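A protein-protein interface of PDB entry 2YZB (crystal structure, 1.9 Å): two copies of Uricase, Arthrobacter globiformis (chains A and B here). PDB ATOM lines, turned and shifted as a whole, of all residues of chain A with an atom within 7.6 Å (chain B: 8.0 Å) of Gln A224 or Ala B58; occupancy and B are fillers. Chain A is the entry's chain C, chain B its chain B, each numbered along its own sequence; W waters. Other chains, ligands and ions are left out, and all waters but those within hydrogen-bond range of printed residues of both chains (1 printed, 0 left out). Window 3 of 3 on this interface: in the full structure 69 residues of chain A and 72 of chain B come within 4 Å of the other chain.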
ATOM      1  N   GLU A 162      -1.484 -34.157  21.071  1.00  0.00           N
ATOM      2  CA  GLU A 162      -1.977 -35.528  21.081  1.00  0.00           C
ATOM      3  C   GLU A 162      -3.452 -35.583  20.706  1.00  0.00           C
ATOM      4  O   GLU A 162      -4.157 -34.577  20.762  1.00  0.00           O
ATOM      5  CB  GLU A 162      -1.843 -36.135  22.478  1.00  0.00           C
ATOM      6  CG  GLU A 162      -0.475 -36.066  23.104  1.00  0.00           C
ATOM      7  CD  GLU A 162      -0.460 -36.741  24.463  1.00  0.00           C
ATOM      8  OE1 GLU A 162      -0.987 -37.867  24.561  1.00  0.00           O
ATOM      9  OE2 GLU A 162       0.076 -36.159  25.427  1.00  0.00           O
ATOM     10  N   ALA A 213      -0.818 -19.195  24.666  1.00  0.00           N
ATOM     11  CA  ALA A 213      -1.646 -20.340  25.019  1.00  0.00           C
ATOM     12  C   ALA A 213      -1.546 -21.454  23.973  1.00  0.00           C
ATOM     13  O   ALA A 213      -1.555 -22.637  24.313  1.00  0.00           O
ATOM     14  CB  ALA A 213      -3.094 -19.904  25.188  1.00  0.00           C
ATOM     15  N   THR A 217       0.341 -24.750  25.786  1.00  0.00           N
ATOM     16  CA  THR A 217      -0.633 -25.745  26.211  1.00  0.00           C
ATOM     17  C   THR A 217      -0.346 -27.105  25.581  1.00  0.00           C
ATOM     18  O   THR A 217      -0.318 -27.230  24.361  1.00  0.00           O
ATOM     19  CB  THR A 217      -2.069 -25.343  25.812  1.00  0.00           C
ATOM     20  OG1 THR A 217      -2.395 -24.075  26.391  1.00  0.00           O
ATOM     21  CG2 THR A 217      -3.068 -26.393  26.289  1.00  0.00           C
ATOM     22  N   HIS A 218      -0.120 -28.120  26.409  1.00  0.00           N
ATOM     23  CA  HIS A 218       0.109 -29.457  25.876  1.00  0.00           C
ATOM     24  C   HIS A 218      -1.260 -29.884  25.369  1.00  0.00           C
ATOM     25  O   HIS A 218      -2.142 -30.230  26.154  1.00  0.00           O
ATOM     26  CB  HIS A 218       0.569 -30.417  26.964  1.00  0.00           C
ATOM     27  CG  HIS A 218       0.889 -31.784  26.447  1.00  0.00           C
ATOM     28  ND1 HIS A 218       1.963 -32.032  25.621  1.00  0.00           N
ATOM     29  CD2 HIS A 218       0.252 -32.968  26.602  1.00  0.00           C
ATOM     30  CE1 HIS A 218       1.976 -33.310  25.288  1.00  0.00           C
ATOM     31  NE2 HIS A 218       0.947 -33.900  25.871  1.00  0.00           N
ATOM     32  N   SER A 219      -1.429 -29.862  24.055  1.00  0.00           N
ATOM     33  CA  SER A 219      -2.706 -30.172  23.432  1.00  0.00           C
ATOM     34  C   SER A 219      -3.145 -31.628  23.401  1.00  0.00           C
ATOM     35  O   SER A 219      -2.424 -32.502  22.916  1.00  0.00           O
ATOM     36  CB  SER A 219      -2.718 -29.609  22.002  1.00  0.00           C
ATOM     37  OG  SER A 219      -4.017 -29.658  21.443  1.00  0.00           O
ATOM     38  N   LEU A 220      -4.343 -31.878  23.924  1.00  0.00           N
ATOM     39  CA  LEU A 220      -4.915 -33.216  23.917  1.00  0.00           C
ATOM     40  C   LEU A 220      -5.985 -33.208  22.830  1.00  0.00           C
ATOM     41  O   LEU A 220      -6.534 -34.246  22.465  1.00  0.00           O
ATOM     42  CB  LEU A 220      -5.547 -33.555  25.273  1.00  0.00           C
ATOM     43  CG  LEU A 220      -4.636 -33.670  26.501  1.00  0.00           C
ATOM     44  CD1 LEU A 220      -5.453 -34.234  27.653  1.00  0.00           C
ATOM     45  CD2 LEU A 220      -3.451 -34.582  26.214  1.00  0.00           C
ATOM     46  N   ALA A 221      -6.259 -32.011  22.318  1.00  0.00           N
ATOM     47  CA  ALA A 221      -7.234 -31.800  21.254  1.00  0.00           C
ATOM     48  C   ALA A 221      -7.239 -30.312  20.897  1.00  0.00           C
ATOM     49  O   ALA A 221      -7.013 -29.462  21.760  1.00  0.00           O
ATOM     50  CB  ALA A 221      -8.621 -32.235  21.714  1.00  0.00           C
ATOM     51  N   LEU A 222      -7.495 -29.990  19.631  1.00  0.00           N
ATOM     52  CA  LEU A 222      -7.516 -28.585  19.218  1.00  0.00           C
ATOM     53  C   LEU A 222      -8.543 -27.837  20.071  1.00  0.00           C
ATOM     54  O   LEU A 222      -8.333 -26.680  20.443  1.00  0.00           O
ATOM     55  CB  LEU A 222      -7.889 -28.460  17.738  1.00  0.00           C
ATOM     56  CG  LEU A 222      -7.139 -27.409  16.903  1.00  0.00           C
ATOM     57  CD1 LEU A 222      -7.973 -27.075  15.680  1.00  0.00           C
ATOM     58  CD2 LEU A 222      -6.874 -26.153  17.706  1.00  0.00           C
ATOM     59  N   GLN A 223      -9.653 -28.512  20.374  1.00  0.00           N
ATOM     60  CA  GLN A 223     -10.718 -27.938  21.192  1.00  0.00           C
ATOM     61  C   GLN A 223     -10.178 -27.433  22.528  1.00  0.00           C
ATOM     62  O   GLN A 223     -10.522 -26.336  22.970  1.00  0.00           O
ATOM     63  CB  GLN A 223     -11.824 -28.974  21.456  1.00  0.00           C
ATOM     64  CG  GLN A 223     -12.731 -29.272  20.262  1.00  0.00           C
ATOM     65  CD  GLN A 223     -12.221 -30.406  19.381  1.00  0.00           C
ATOM     66  OE1 GLN A 223     -11.016 -30.575  19.198  1.00  0.00           O
ATOM     67  NE2 GLN A 223     -13.148 -31.179  18.818  1.00  0.00           N
ATOM     68  N   GLN A 224      -9.334 -28.239  23.168  1.00  0.00           N
ATOM     69  CA  GLN A 224      -8.752 -27.872  24.458  1.00  0.00           C
ATOM     70  C   GLN A 224      -7.814 -26.681  24.302  1.00  0.00           C
ATOM     71  O   GLN A 224      -7.788 -25.783  25.141  1.00  0.00           O
ATOM     72  CB  GLN A 224      -7.976 -29.053  25.054  1.00  0.00           C
ATOM     73  CG  GLN A 224      -7.626 -28.869  26.522  1.00  0.00           C
ATOM     74  CD  GLN A 224      -6.443 -29.714  26.960  1.00  0.00           C
ATOM     75  OE1 GLN A 224      -6.225 -29.922  28.155  1.00  0.00           O
ATOM     76  NE2 GLN A 224      -5.663 -30.195  25.994  1.00  0.00           N
ATOM     77  N   THR A 225      -7.032 -26.686  23.226  1.00  0.00           N
ATOM     78  CA  THR A 225      -6.107 -25.594  22.960  1.00  0.00           C
ATOM     79  C   THR A 225      -6.881 -24.299  22.713  1.00  0.00           C
ATOM     80  O   THR A 225      -6.496 -23.228  23.191  1.00  0.00           O
ATOM     81  CB  THR A 225      -5.236 -25.901  21.726  1.00  0.00           C
ATOM     82  OG1 THR A 225      -4.386 -27.018  22.018  1.00  0.00           O
ATOM     83  CG2 THR A 225      -4.387 -24.697  21.349  1.00  0.00           C
ATOM     84  N   MET A 226      -7.976 -24.404  21.970  1.00  0.00           N
ATOM     85  CA  MET A 226      -8.786 -23.237  21.669  1.00  0.00           C
ATOM     86  C   MET A 226      -9.411 -22.687  22.944  1.00  0.00           C
ATOM     87  O   MET A 226      -9.481 -21.475  23.131  1.00  0.00           O
ATOM     88  CB  MET A 226      -9.880 -23.586  20.658  1.00  0.00           C
ATOM     89  CG  MET A 226     -10.762 -22.398  20.297  1.00  0.00           C
ATOM     90  SD  MET A 226     -11.933 -22.776  18.986  1.00  0.00           S
ATOM     91  CE  MET A 226     -12.808 -24.141  19.728  1.00  0.00           C
ATOM     92  N   TYR A 227      -9.862 -23.582  23.816  1.00  0.00           N
ATOM     93  CA  TYR A 227     -10.470 -23.178  25.077  1.00  0.00           C
ATOM     94  C   TYR A 227      -9.456 -22.431  25.938  1.00  0.00           C
ATOM     95  O   TYR A 227      -9.772 -21.401  26.535  1.00  0.00           O
ATOM     96  CB  TYR A 227     -10.976 -24.407  25.841  1.00  0.00           C
ATOM     97  CG  TYR A 227     -11.565 -24.081  27.196  1.00  0.00           C
ATOM     98  CD1 TYR A 227     -12.842 -23.526  27.313  1.00  0.00           C
ATOM     99  CD2 TYR A 227     -10.835 -24.307  28.364  1.00  0.00           C
ATOM    100  CE1 TYR A 227     -13.376 -23.205  28.563  1.00  0.00           C
ATOM    101  CE2 TYR A 227     -11.357 -23.988  29.616  1.00  0.00           C
ATOM    102  CZ  TYR A 227     -12.625 -23.438  29.710  1.00  0.00           C
ATOM    103  OH  TYR A 227     -13.133 -23.117  30.950  1.00  0.00           O
ATOM    104  N   GLU A 228      -8.233 -22.947  25.999  1.00  0.00           N
ATOM    105  CA  GLU A 228      -7.202 -22.308  26.806  1.00  0.00           C
ATOM    106  C   GLU A 228      -6.837 -20.932  26.264  1.00  0.00           C
ATOM    107  O   GLU A 228      -6.564 -20.008  27.035  1.00  0.00           O
ATOM    108  CB  GLU A 228      -5.958 -23.199  26.879  1.00  0.00           C
ATOM    109  CG  GLU A 228      -6.212 -24.515  27.594  1.00  0.00           C
ATOM    110  CD  GLU A 228      -6.734 -24.315  29.012  1.00  0.00           C
ATOM    111  OE1 GLU A 228      -7.414 -25.224  29.534  1.00  0.00           O
ATOM    112  OE2 GLU A 228      -6.458 -23.253  29.608  1.00  0.00           O
ATOM    113  N   MET A 229      -6.829 -20.796  24.941  1.00  0.00           N
ATOM    114  CA  MET A 229      -6.510 -19.519  24.312  1.00  0.00           C
ATOM    115  C   MET A 229      -7.562 -18.492  24.715  1.00  0.00           C
ATOM    116  O   MET A 229      -7.234 -17.387  25.136  1.00  0.00           O
ATOM    117  CB  MET A 229      -6.470 -19.677  22.786  1.00  0.00           C
ATOM    118  CG  MET A 229      -5.248 -20.450  22.284  1.00  0.00           C
ATOM    119  SD  MET A 229      -5.375 -21.061  20.572  1.00  0.00           S
ATOM    120  CE  MET A 229      -5.241 -19.517  19.654  1.00  0.00           C
ATOM    121  N   GLY A 230      -8.828 -18.877  24.602  1.00  0.00           N
ATOM    122  CA  GLY A 230      -9.910 -17.981  24.964  1.00  0.00           C
ATOM    123  C   GLY A 230      -9.937 -17.665  26.445  1.00  0.00           C
ATOM    124  O   GLY A 230     -10.109 -16.511  26.836  1.00  0.00           O
ATOM    125  N   ARG A 231      -9.755 -18.689  27.276  1.00  0.00           N
ATOM    126  CA  ARG A 231      -9.771 -18.502  28.722  1.00  0.00           C
ATOM    127  C   ARG A 231      -8.748 -17.451  29.131  1.00  0.00           C
ATOM    128  O   ARG A 231      -9.032 -16.574  29.947  1.00  0.00           O
ATOM    129  CB  ARG A 231      -9.470 -19.824  29.441  1.00  0.00           C
ATOM    130  CG  ARG A 231      -9.701 -19.760  30.948  1.00  0.00           C
ATOM    131  CD  ARG A 231      -9.278 -21.036  31.675  1.00  0.00           C
ATOM    132  NE  ARG A 231      -7.830 -21.113  31.868  1.00  0.00           N
ATOM    133  CZ  ARG A 231      -7.207 -22.113  32.488  1.00  0.00           C
ATOM    134  NH1 ARG A 231      -7.900 -23.131  32.978  1.00  0.00           N
ATOM    135  NH2 ARG A 231      -5.887 -22.097  32.620  1.00  0.00           N
ATOM    136  N   ILE A 279     -12.526 -26.362  13.901  1.00  0.00           N
ATOM    137  CA  ILE A 279     -12.991 -26.318  15.277  1.00  0.00           C
ATOM    138  C   ILE A 279     -13.330 -24.874  15.642  1.00  0.00           C
ATOM    139  O   ILE A 279     -12.498 -23.978  15.500  1.00  0.00           O
ATOM    140  CB  ILE A 279     -11.894 -26.881  16.230  1.00  0.00           C
ATOM    141  CG1 ILE A 279     -11.827 -28.413  16.121  1.00  0.00           C
ATOM    142  CG2 ILE A 279     -12.199 -26.510  17.665  1.00  0.00           C
ATOM    143  CD1 ILE A 279     -11.528 -28.959  14.735  1.00  0.00           C
ATOM    144  N   PHE B  52     -19.948 -31.079  24.265  1.00  0.00           N
ATOM    145  CA  PHE B  52     -18.515 -31.227  24.058  1.00  0.00           C
ATOM    146  C   PHE B  52     -17.750 -30.456  25.131  1.00  0.00           C
ATOM    147  O   PHE B  52     -16.598 -30.067  24.938  1.00  0.00           O
ATOM    148  CB  PHE B  52     -18.143 -30.728  22.661  1.00  0.00           C
ATOM    149  CG  PHE B  52     -18.853 -31.459  21.554  1.00  0.00           C
ATOM    150  CD1 PHE B  52     -19.677 -30.774  20.667  1.00  0.00           C
ATOM    151  CD2 PHE B  52     -18.713 -32.837  21.409  1.00  0.00           C
ATOM    152  CE1 PHE B  52     -20.358 -31.450  19.647  1.00  0.00           C
ATOM    153  CE2 PHE B  52     -19.389 -33.523  20.395  1.00  0.00           C
ATOM    154  CZ  PHE B  52     -20.213 -32.824  19.512  1.00  0.00           C
ATOM    155  N   GLU B  53     -18.410 -30.253  26.268  1.00  0.00           N
ATOM    156  CA  GLU B  53     -17.843 -29.532  27.408  1.00  0.00           C
ATOM    157  C   GLU B  53     -16.492 -30.094  27.871  1.00  0.00           C
ATOM    158  O   GLU B  53     -15.505 -29.363  27.960  1.00  0.00           O
ATOM    159  CB  GLU B  53     -18.848 -29.563  28.571  1.00  0.00           C
ATOM    160  CG  GLU B  53     -18.449 -28.781  29.821  1.00  0.00           C
ATOM    161  CD  GLU B  53     -18.575 -27.277  29.646  1.00  0.00           C
ATOM    162  OE1 GLU B  53     -19.508 -26.839  28.939  1.00  0.00           O
ATOM    163  OE2 GLU B  53     -17.756 -26.532  30.226  1.00  0.00           O
ATOM    164  N   ALA B  54     -16.445 -31.389  28.164  1.00  0.00           N
ATOM    165  CA  ALA B  54     -15.211 -32.022  28.632  1.00  0.00           C
ATOM    166  C   ALA B  54     -14.094 -31.980  27.594  1.00  0.00           C
ATOM    167  O   ALA B  54     -12.912 -31.936  27.941  1.00  0.00           O
ATOM    168  CB  ALA B  54     -15.487 -33.462  29.044  1.00  0.00           C
ATOM    169  N   ALA B  55     -14.466 -32.004  26.320  1.00  0.00           N
ATOM    170  CA  ALA B  55     -13.479 -31.953  25.248  1.00  0.00           C
ATOM    171  C   ALA B  55     -12.703 -30.644  25.333  1.00  0.00           C
ATOM    172  O   ALA B  55     -11.472 -30.634  25.258  1.00  0.00           O
ATOM    173  CB  ALA B  55     -14.167 -32.068  23.890  1.00  0.00           C
ATOM    174  N   HIS B  56     -13.424 -29.539  25.508  1.00  0.00           N
ATOM    175  CA  HIS B  56     -12.784 -28.232  25.584  1.00  0.00           C
ATOM    176  C   HIS B  56     -12.100 -27.943  26.920  1.00  0.00           C
ATOM    177  O   HIS B  56     -10.972 -27.454  26.949  1.00  0.00           O
ATOM    178  CB  HIS B  56     -13.798 -27.111  25.300  1.00  0.00           C
ATOM    179  CG  HIS B  56     -14.364 -27.130  23.912  1.00  0.00           C
ATOM    180  ND1 HIS B  56     -15.354 -28.005  23.519  1.00  0.00           N
ATOM    181  CD2 HIS B  56     -14.070 -26.380  22.821  1.00  0.00           C
ATOM    182  CE1 HIS B  56     -15.649 -27.792  22.248  1.00  0.00           C
ATOM    183  NE2 HIS B  56     -14.885 -26.812  21.802  1.00  0.00           N
ATOM    184  N   THR B  57     -12.771 -28.255  28.026  1.00  0.00           N
ATOM    185  CA  THR B  57     -12.219 -27.966  29.348  1.00  0.00           C
ATOM    186  C   THR B  57     -11.164 -28.925  29.903  1.00  0.00           C
ATOM    187  O   THR B  57     -10.275 -28.503  30.642  1.00  0.00           O
ATOM    188  CB  THR B  57     -13.352 -27.836  30.391  1.00  0.00           C
ATOM    189  OG1 THR B  57     -14.018 -29.097  30.539  1.00  0.00           O
ATOM    190  CG2 THR B  57     -14.364 -26.781  29.943  1.00  0.00           C
ATOM    191  N   ALA B  58     -11.248 -30.205  29.556  1.00  0.00           N
ATOM    192  CA  ALA B  58     -10.284 -31.177  30.064  1.00  0.00           C
ATOM    193  C   ALA B  58      -9.554 -31.956  28.971  1.00  0.00           C
ATOM    194  O   ALA B  58      -8.559 -32.632  29.236  1.00  0.00           O
ATOM    195  CB  ALA B  58     -10.983 -32.146  31.004  1.00  0.00           C
ATOM    196  N   GLY B  59     -10.046 -31.868  27.743  1.00  0.00           N
ATOM    197  CA  GLY B  59      -9.406 -32.593  26.662  1.00  0.00           C
ATOM    198  C   GLY B  59      -9.872 -34.035  26.592  1.00  0.00           C
ATOM    199  O   GLY B  59      -9.216 -34.874  25.973  1.00  0.00           O
ATOM    200  N   ASP B  60     -10.997 -34.329  27.241  1.00  0.00           N
ATOM    201  CA  ASP B  60     -11.556 -35.678  27.219  1.00  0.00           C
ATOM    202  C   ASP B  60     -12.290 -35.822  25.890  1.00  0.00           C
ATOM    203  O   ASP B  60     -13.322 -35.188  25.666  1.00  0.00           O
ATOM    204  CB  ASP B  60     -12.514 -35.878  28.401  1.00  0.00           C
ATOM    205  CG  ASP B  60     -13.328 -37.156  28.286  1.00  0.00           C
ATOM    206  OD1 ASP B  60     -12.802 -38.152  27.748  1.00  0.00           O
ATOM    207  OD2 ASP B  60     -14.494 -37.170  28.742  1.00  0.00           O
ATOM    208  N   ASN B  61     -11.749 -36.658  25.010  1.00  0.00           N
ATOM    209  CA  ASN B  61     -12.320 -36.852  23.685  1.00  0.00           C
ATOM    210  C   ASN B  61     -13.361 -37.954  23.553  1.00  0.00           C
ATOM    211  O   ASN B  61     -13.700 -38.362  22.440  1.00  0.00           O
ATOM    212  CB  ASN B  61     -11.190 -37.080  22.678  1.00  0.00           C
ATOM    213  CG  ASN B  61     -10.221 -35.924  22.641  1.00  0.00           C
ATOM    214  OD1 ASN B  61     -10.632 -34.763  22.604  1.00  0.00           O
ATOM    215  ND2 ASN B  61      -8.927 -36.229  22.651  1.00  0.00           N
HETATM  216  O   HOH W   1      -5.960 -36.745  23.207  1.00  0.00           O
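CD1 of Leu A220 touches O of Ala B58, at 3.8 Å.
O of Gly B59 touches CB of Leu A220, at 3.96 Å.
Ala A221 touches Asn B61.
Gln A223 touches His B56.
Ala B55 touches Gln A224.
His B56 touches Gln A224.
O of Ala B58 touches OE1 of Gln A224, at 3.7 Å.
CE of Met A226 touches NE2 of His B56, 3.97 Å away.
Tyr A227 touches His B56.
Tyr A227 touches Thr B57.
Gln A224 touches three residues of chain B.
Of chain A, only Leu A220 and Gln A224 come within 4 Å of Ala B58.
Of the printed residues of chain A, Asn B61 touches Leu A220 (3.1 Å) and Ala A221 (3.4 Å).
Printed residues of chain A within 4 Å of Ala B55: Gln A224.
Of the printed residues of chain A, His B56 touches Gln A223 (3.6 Å), Gln A224 (3.4 Å), Met A226 (3.97 Å) and Tyr A227 (3.2 Å).
Printed residues of chain A within 4 Å of Thr B57: Tyr A227 (3.8 Å).
The nearest printed residue of chain B that does not touch Tyr A227 is Glu B53 (5.7 Å).
Water W1 bridges O of Leu A220 and ND2 of Asn B61.
A ring nitrogen (ND1) of His B56 sits at hydrogen-bond distance from the backbone carbonyl oxygen of Phe B52.
The side-chain hydroxyl (OG1) of Thr B57 lies within hydrogen-bond range of the backbone carbonyl oxygen (O) of Glu B53, at 3.0 Å.
N of Gly B59 sits at hydrogen-bond distance from O of Ala B54, at 2.9 Å.
The backbone NH of Ala B55 sits close to the backbone carbonyl oxygen of Asp B60, 3.4 Å away.
The side-chain hydroxyl of Ser A219 sits at hydrogen-bond distance from the backbone carbonyl oxygen of Ala A221 (3.0 Å).
N of Leu A220 sits close to NE2 of Gln A224 (3.0 Å).
Printed residues of chain B that touch a printed residue of chain A: Ala B55, His B56, Thr B57, Ala B58, Gly B59 and Asn B61.
Hydrophobic or aromatic side chains of chain B within 4 Å of the printed part of chain A: His B56.
Among the printed residues, no Asp or Glu carboxylate lies within 4 Å of a Lys or Arg side-chain nitrogen of the other chain.
No position is printed for both chains.
The side-chain amide nitrogen of Asn B61 lies within hydrogen-bond range of the backbone carbonyl oxygen of Leu A220 (3.1 Å).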
